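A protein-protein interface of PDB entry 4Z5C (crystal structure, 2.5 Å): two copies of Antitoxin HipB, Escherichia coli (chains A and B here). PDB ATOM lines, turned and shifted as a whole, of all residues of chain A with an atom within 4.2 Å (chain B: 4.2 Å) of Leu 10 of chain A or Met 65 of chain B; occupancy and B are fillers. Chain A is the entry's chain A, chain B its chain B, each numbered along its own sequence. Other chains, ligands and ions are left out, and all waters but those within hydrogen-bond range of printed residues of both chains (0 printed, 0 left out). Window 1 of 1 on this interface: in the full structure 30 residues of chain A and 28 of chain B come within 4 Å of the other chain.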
ATOM      1  N   LYS A   3      22.971 -15.585 -26.742  1.00  0.00           N
ATOM      2  CA  LYS A   3      22.928 -15.144 -25.354  1.00  0.00           C
ATOM      3  C   LYS A   3      21.537 -14.692 -24.919  1.00  0.00           C
ATOM      4  O   LYS A   3      20.815 -14.046 -25.676  1.00  0.00           O
ATOM      5  CB  LYS A   3      23.966 -14.054 -25.097  1.00  0.00           C
ATOM      6  CG  LYS A   3      25.380 -14.476 -25.484  1.00  0.00           C
ATOM      7  CD  LYS A   3      26.388 -13.344 -25.310  1.00  0.00           C
ATOM      8  CE  LYS A   3      27.816 -13.861 -25.350  1.00  0.00           C
ATOM      9  NZ  LYS A   3      28.807 -12.754 -25.238  1.00  0.00           N
ATOM     10  N   ILE A   4      21.177 -15.052 -23.689  1.00  0.00           N
ATOM     11  CA  ILE A   4      19.854 -14.783 -23.134  1.00  0.00           C
ATOM     12  C   ILE A   4      19.919 -13.797 -21.972  1.00  0.00           C
ATOM     13  O   ILE A   4      20.785 -13.897 -21.106  1.00  0.00           O
ATOM     14  CB  ILE A   4      19.164 -16.099 -22.723  1.00  0.00           C
ATOM     15  CG1 ILE A   4      18.747 -16.854 -23.991  1.00  0.00           C
ATOM     16  CG2 ILE A   4      17.961 -15.829 -21.812  1.00  0.00           C
ATOM     17  CD1 ILE A   4      18.488 -18.290 -23.776  1.00  0.00           C
ATOM     18  N   SER A   6      16.878 -12.239 -20.312  1.00  0.00           N
ATOM     19  CA  SER A   6      15.690 -12.078 -19.475  1.00  0.00           C
ATOM     20  C   SER A   6      14.929 -13.389 -19.360  1.00  0.00           C
ATOM     21  O   SER A   6      15.113 -14.284 -20.188  1.00  0.00           O
ATOM     22  CB  SER A   6      14.769 -10.999 -20.064  1.00  0.00           C
ATOM     23  OG  SER A   6      14.297 -11.380 -21.351  1.00  0.00           O
ATOM     24  N   PRO A   7      14.070 -13.508 -18.329  1.00  0.00           N
ATOM     25  CA  PRO A   7      13.171 -14.659 -18.172  1.00  0.00           C
ATOM     26  C   PRO A   7      12.271 -14.888 -19.392  1.00  0.00           C
ATOM     27  O   PRO A   7      12.135 -16.029 -19.837  1.00  0.00           O
ATOM     28  CB  PRO A   7      12.316 -14.271 -16.960  1.00  0.00           C
ATOM     29  CG  PRO A   7      13.203 -13.388 -16.161  1.00  0.00           C
ATOM     30  CD  PRO A   7      13.990 -12.593 -17.174  1.00  0.00           C
ATOM     31  N   THR A   8      11.674 -13.815 -19.917  1.00  0.00           N
ATOM     32  CA  THR A   8      10.798 -13.887 -21.089  1.00  0.00           C
ATOM     33  C   THR A   8      11.536 -14.492 -22.262  1.00  0.00           C
ATOM     34  O   THR A   8      11.047 -15.405 -22.925  1.00  0.00           O
ATOM     35  CB  THR A   8      10.328 -12.494 -21.517  1.00  0.00           C
ATOM     36  OG1 THR A   8       9.300 -12.041 -20.631  1.00  0.00           O
ATOM     37  CG2 THR A   8       9.789 -12.520 -22.934  1.00  0.00           C
ATOM     38  N   GLN A   9      12.728 -13.972 -22.513  1.00  0.00           N
ATOM     39  CA  GLN A   9      13.563 -14.479 -23.584  1.00  0.00           C
ATOM     40  C   GLN A   9      13.924 -15.955 -23.336  1.00  0.00           C
ATOM     41  O   GLN A   9      13.895 -16.775 -24.255  1.00  0.00           O
ATOM     42  CB  GLN A   9      14.808 -13.601 -23.737  1.00  0.00           C
ATOM     43  CG  GLN A   9      15.533 -13.822 -25.042  1.00  0.00           C
ATOM     44  CD  GLN A   9      16.938 -13.261 -25.044  1.00  0.00           C
ATOM     45  OE1 GLN A   9      17.244 -12.300 -24.323  1.00  0.00           O
ATOM     46  NE2 GLN A   9      17.809 -13.864 -25.856  1.00  0.00           N
ATOM     47  N   LEU A  10      14.238 -16.296 -22.091  1.00  0.00           N
ATOM     48  CA  LEU A  10      14.591 -17.673 -21.752  1.00  0.00           C
ATOM     49  C   LEU A  10      13.413 -18.609 -21.999  1.00  0.00           C
ATOM     50  O   LEU A  10      13.558 -19.643 -22.651  1.00  0.00           O
ATOM     51  CB  LEU A  10      15.045 -17.759 -20.293  1.00  0.00           C
ATOM     52  CG  LEU A  10      15.297 -19.141 -19.686  1.00  0.00           C
ATOM     53  CD1 LEU A  10      16.589 -19.764 -20.188  1.00  0.00           C
ATOM     54  CD2 LEU A  10      15.308 -19.025 -18.172  1.00  0.00           C
ATOM     55  N   ALA A  11      12.247 -18.239 -21.475  1.00  0.00           N
ATOM     56  CA  ALA A  11      11.035 -19.025 -21.661  1.00  0.00           C
ATOM     57  C   ALA A  11      10.716 -19.193 -23.139  1.00  0.00           C
ATOM     58  O   ALA A  11      10.356 -20.287 -23.584  1.00  0.00           O
ATOM     59  CB  ALA A  11       9.878 -18.377 -20.953  1.00  0.00           C
ATOM     60  N   ASN A  12      10.859 -18.111 -23.900  1.00  0.00           N
ATOM     61  CA  ASN A  12      10.560 -18.153 -25.326  1.00  0.00           C
ATOM     62  C   ASN A  12      11.436 -19.156 -26.040  1.00  0.00           C
ATOM     63  O   ASN A  12      10.957 -19.958 -26.848  1.00  0.00           O
ATOM     64  CB  ASN A  12      10.710 -16.769 -25.969  1.00  0.00           C
ATOM     65  CG  ASN A  12       9.610 -15.821 -25.559  1.00  0.00           C
ATOM     66  OD1 ASN A  12       8.513 -16.253 -25.180  1.00  0.00           O
ATOM     67  ND2 ASN A  12       9.891 -14.521 -25.615  1.00  0.00           N
ATOM     68  N   ALA A  13      12.724 -19.120 -25.721  1.00  0.00           N
ATOM     69  CA  ALA A  13      13.682 -20.027 -26.336  1.00  0.00           C
ATOM     70  C   ALA A  13      13.325 -21.478 -26.019  1.00  0.00           C
ATOM     71  O   ALA A  13      13.342 -22.344 -26.902  1.00  0.00           O
ATOM     72  CB  ALA A  13      15.090 -19.697 -25.879  1.00  0.00           C
ATOM     73  N   MET A  14      12.976 -21.725 -24.758  1.00  0.00           N
ATOM     74  CA  MET A  14      12.682 -23.079 -24.299  1.00  0.00           C
ATOM     75  C   MET A  14      11.394 -23.609 -24.912  1.00  0.00           C
ATOM     76  O   MET A  14      11.329 -24.769 -25.317  1.00  0.00           O
ATOM     77  CB  MET A  14      12.670 -23.150 -22.762  1.00  0.00           C
ATOM     78  CG  MET A  14      14.075 -23.269 -22.189  1.00  0.00           C
ATOM     79  SD  MET A  14      14.264 -22.834 -20.459  1.00  0.00           S
ATOM     80  CE  MET A  14      13.684 -24.342 -19.681  1.00  0.00           C
ATOM     81  N   PHE A  54      12.939 -24.063 -13.328  1.00  0.00           N
ATOM     82  CA  PHE A  54      13.700 -23.798 -14.548  1.00  0.00           C
ATOM     83  C   PHE A  54      14.608 -24.976 -14.896  1.00  0.00           C
ATOM     84  O   PHE A  54      14.646 -25.423 -16.044  1.00  0.00           O
ATOM     85  CB  PHE A  54      14.490 -22.488 -14.416  1.00  0.00           C
ATOM     86  CG  PHE A  54      15.658 -22.366 -15.368  1.00  0.00           C
ATOM     87  CD1 PHE A  54      15.494 -22.521 -16.736  1.00  0.00           C
ATOM     88  CD2 PHE A  54      16.922 -22.054 -14.889  1.00  0.00           C
ATOM     89  CE1 PHE A  54      16.584 -22.405 -17.603  1.00  0.00           C
ATOM     90  CE2 PHE A  54      18.009 -21.933 -15.752  1.00  0.00           C
ATOM     91  CZ  PHE A  54      17.841 -22.113 -17.104  1.00  0.00           C
ATOM     92  N   MET A  65      22.593 -25.471 -19.465  1.00  0.00           N
ATOM     93  CA  MET A  65      22.938 -24.073 -19.665  1.00  0.00           C
ATOM     94  C   MET A  65      24.399 -23.837 -19.345  1.00  0.00           C
ATOM     95  O   MET A  65      25.043 -24.645 -18.680  1.00  0.00           O
ATOM     96  CB  MET A  65      22.078 -23.176 -18.776  1.00  0.00           C
ATOM     97  CG  MET A  65      22.346 -23.369 -17.305  1.00  0.00           C
ATOM     98  SD  MET A  65      21.995 -21.886 -16.363  1.00  0.00           S
ATOM     99  CE  MET A  65      23.445 -20.914 -16.696  1.00  0.00           C
ATOM    100  N   THR A  66      24.911 -22.708 -19.807  1.00  0.00           N
ATOM    101  CA  THR A  66      26.297 -22.355 -19.580  1.00  0.00           C
ATOM    102  C   THR A  66      26.391 -20.855 -19.348  1.00  0.00           C
ATOM    103  O   THR A  66      25.626 -20.079 -19.922  1.00  0.00           O
ATOM    104  CB  THR A  66      27.183 -22.763 -20.780  1.00  0.00           C
ATOM    105  OG1 THR A  66      28.562 -22.567 -20.452  1.00  0.00           O
ATOM    106  CG2 THR A  66      26.834 -21.940 -22.016  1.00  0.00           C
ATOM    107  N   CYS A  68      28.404 -17.136 -19.521  1.00  0.00           N
ATOM    108  CA  CYS A  68      29.283 -16.467 -20.482  1.00  0.00           C
ATOM    109  C   CYS A  68      29.329 -14.956 -20.265  1.00  0.00           C
ATOM    110  O   CYS A  68      28.530 -14.409 -19.509  1.00  0.00           O
ATOM    111  CB  CYS A  68      28.867 -16.780 -21.921  1.00  0.00           C
ATOM    112  SG  CYS A  68      27.343 -15.981 -22.438  1.00  0.00           S
ATOM    113  N   LEU B  51      13.489 -16.162 -11.304  1.00  0.00           N
ATOM    114  CA  LEU B  51      14.241 -15.947 -12.521  1.00  0.00           C
ATOM    115  C   LEU B  51      14.630 -14.470 -12.712  1.00  0.00           C
ATOM    116  O   LEU B  51      15.684 -14.179 -13.271  1.00  0.00           O
ATOM    117  CB  LEU B  51      13.483 -16.498 -13.731  1.00  0.00           C
ATOM    118  CG  LEU B  51      13.432 -18.028 -13.882  1.00  0.00           C
ATOM    119  CD1 LEU B  51      12.887 -18.444 -15.245  1.00  0.00           C
ATOM    120  CD2 LEU B  51      14.798 -18.642 -13.669  1.00  0.00           C
ATOM    121  N   PHE B  55      18.614 -13.118 -13.345  1.00  0.00           N
ATOM    122  CA  PHE B  55      19.066 -12.317 -14.476  1.00  0.00           C
ATOM    123  C   PHE B  55      19.632 -10.956 -14.067  1.00  0.00           C
ATOM    124  O   PHE B  55      20.566 -10.451 -14.703  1.00  0.00           O
ATOM    125  CB  PHE B  55      17.969 -12.217 -15.541  1.00  0.00           C
ATOM    126  CG  PHE B  55      17.858 -13.445 -16.391  1.00  0.00           C
ATOM    127  CD1 PHE B  55      18.762 -13.668 -17.425  1.00  0.00           C
ATOM    128  CD2 PHE B  55      16.874 -14.390 -16.154  1.00  0.00           C
ATOM    129  CE1 PHE B  55      18.673 -14.811 -18.220  1.00  0.00           C
ATOM    130  CE2 PHE B  55      16.780 -15.545 -16.944  1.00  0.00           C
ATOM    131  CZ  PHE B  55      17.679 -15.750 -17.976  1.00  0.00           C
ATOM    132  N   LEU B  58      23.078 -11.834 -12.553  1.00  0.00           N
ATOM    133  CA  LEU B  58      23.872 -12.244 -13.704  1.00  0.00           C
ATOM    134  C   LEU B  58      24.429 -11.015 -14.418  1.00  0.00           C
ATOM    135  O   LEU B  58      25.612 -10.947 -14.737  1.00  0.00           O
ATOM    136  CB  LEU B  58      22.988 -13.051 -14.654  1.00  0.00           C
ATOM    137  CG  LEU B  58      23.608 -13.870 -15.780  1.00  0.00           C
ATOM    138  CD1 LEU B  58      24.707 -14.777 -15.245  1.00  0.00           C
ATOM    139  CD2 LEU B  58      22.516 -14.695 -16.474  1.00  0.00           C
ATOM    140  N   SER B  64      26.319 -13.368 -19.051  1.00  0.00           N
ATOM    141  CA  SER B  64      25.079 -13.794 -19.674  1.00  0.00           C
ATOM    142  C   SER B  64      25.012 -15.312 -19.638  1.00  0.00           C
ATOM    143  O   SER B  64      25.843 -15.960 -19.014  1.00  0.00           O
ATOM    144  CB  SER B  64      24.984 -13.305 -21.115  1.00  0.00           C
ATOM    145  OG  SER B  64      23.702 -13.607 -21.646  1.00  0.00           O
ATOM    146  N   MET B  65      24.015 -15.881 -20.299  1.00  0.00           N
ATOM    147  CA  MET B  65      23.907 -17.324 -20.373  1.00  0.00           C
ATOM    148  C   MET B  65      23.349 -17.711 -21.723  1.00  0.00           C
ATOM    149  O   MET B  65      22.662 -16.916 -22.357  1.00  0.00           O
ATOM    150  CB  MET B  65      23.000 -17.847 -19.257  1.00  0.00           C
ATOM    151  CG  MET B  65      21.590 -17.271 -19.268  1.00  0.00           C
ATOM    152  SD  MET B  65      20.312 -18.539 -19.098  1.00  0.00           S
ATOM    153  CE  MET B  65      20.216 -19.171 -20.755  1.00  0.00           C
ATOM    154  N   THR B  66      23.667 -18.916 -22.178  1.00  0.00           N
ATOM    155  CA  THR B  66      22.989 -19.484 -23.335  1.00  0.00           C
ATOM    156  C   THR B  66      22.525 -20.884 -22.958  1.00  0.00           C
ATOM    157  O   THR B  66      22.951 -21.440 -21.937  1.00  0.00           O
ATOM    158  CB  THR B  66      23.904 -19.573 -24.575  1.00  0.00           C
ATOM    159  OG1 THR B  66      24.904 -20.572 -24.356  1.00  0.00           O
ATOM    160  CG2 THR B  66      24.586 -18.240 -24.854  1.00  0.00           C
ATOM    161  N   LEU B  67      21.638 -21.448 -23.770  1.00  0.00           N
ATOM    162  CA  LEU B  67      21.236 -22.836 -23.595  1.00  0.00           C
ATOM    163  C   LEU B  67      22.176 -23.701 -24.418  1.00  0.00           C
ATOM    164  O   LEU B  67      22.828 -23.218 -25.347  1.00  0.00           O
ATOM    165  CB  LEU B  67      19.784 -23.040 -24.038  1.00  0.00           C
ATOM    166  CG  LEU B  67      18.766 -22.179 -23.291  1.00  0.00           C
ATOM    167  CD1 LEU B  67      17.400 -22.210 -23.945  1.00  0.00           C
ATOM    168  CD2 LEU B  67      18.676 -22.619 -21.850  1.00  0.00           C
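O of Ile 4 of chain A touches CE1 of Phe 55 of chain B (3.7 Å). CG of Leu 67 of chain B touches CD1 of Ile 4 of chain A, at 3.9 Å. Pro 7 of chain A touches Phe 55 of chain B. CD1 of Leu 51 of chain B touches CD2 of Leu 10 of chain A (3.8 Å). Leu 10 of chain A touches Phe 55 of chain B. CD1 of Leu 10 of chain A touches CD2 of Leu 67 of chain B, 3.9 Å away. CB of Ala 13 of chain A touches CD1 of Leu 67 of chain B, 3.9 Å away. Met 14 of chain A touches Leu 67 of chain B. O of Thr 66 of chain B touches CA of Met 65 of chain A, 3.5 Å away. Thr 66 of chain A touches Met 65 of chain B.
Of the printed residues of chain B, Ser 6 of chain A touches Phe 55 (3.7 Å). Printed residues of chain B within 4 Å of Pro 7 of chain A: Leu 51 (3.9 Å) and Phe 55 (3.5 Å). Leu 10 of chain A touches four residues of chain B. Ala 11 of chain A touches none of the printed residues of chain B. Of the printed residues of chain B, Ala 13 of chain A touches Leu 67 (3.9 Å). Of the printed residues of chain A, Phe 55 of chain B touches Ile 4 (3.7 Å), Ser 6 (3.7 Å), Pro 7 (3.5 Å) and Leu 10 (3.97 Å). Leu 58 of chain B touches none of the printed residues of chain A. Of chain A, only Lys 3, Ile 4, Leu 10, Thr 66 and Cys 68 come within 4 Å of Met 65 of chain B. Printed residues of chain A within 4 Å of Thr 66 of chain B: Lys 3 (3.5 Å), Met 65 (3.5 Å) and Thr 66 (3.2 Å). The nearest printed residue of chain B that does not touch Leu 10 of chain A is Thr 66 of chain B (6.6 Å). The nearest residue of chain A that does not touch Met 65 of chain B is Met 65 of chain A (4.02 Å).
Met 65 of chain A touches Thr 66 of chain B, and with the chains exchanged Thr 66 of chain A touches Met 65 of chain B. Thr 66 of chain B touches its own counterpart, Thr 66 of chain A. 2 positions are printed for both chains. Of the 22 pairs that touch across the chains among the printed residues, 3 have their exchanged pair printed and touching as well.
O of Lys 3 of chain A sits at hydrogen-bond distance from NE2 of Gln 9 of chain A, 3.0 Å away. N of Gln 9 of chain A is in hydrogen-bond range of OG of Ser 6 of chain A (3.2 Å).
Hydrophobic or aromatic side chains of chain A within 4 Å of the printed part of chain B: Ile 4, Pro 7, Leu 10, Ala 13, Met 14, Phe 54 and Met 65. Printed residues of chain B that touch a printed residue of chain A: Leu 51, Phe 55, Ser 64, Met 65, Thr 66 and Leu 67. Hydrophobic or aromatic side chains of chain B within 4 Å of the printed part of chain A: Leu 51, Phe 55, Met 65 and Leu 67. Among the printed residues, 22 pairs touch across the chains.
N of Thr 66 of chain A lies within hydrogen-bond range of O of Thr 66 of chain B (3.2 Å). The backbone carbonyl oxygen (O) of Met 65 of chain B sits at hydrogen-bond distance from the backbone NH (N) of Ile 4 of chain A, 2.7 Å away. The backbone carbonyl oxygen of Ile 4 of chain A is in hydrogen-bond range of the side-chain hydroxyl of Ser 64 of chain B, at 3.0 Å. O of Cys 68 of chain A sits at hydrogen-bond distance from N of Ser 64 of chain B, at 2.5 Å.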
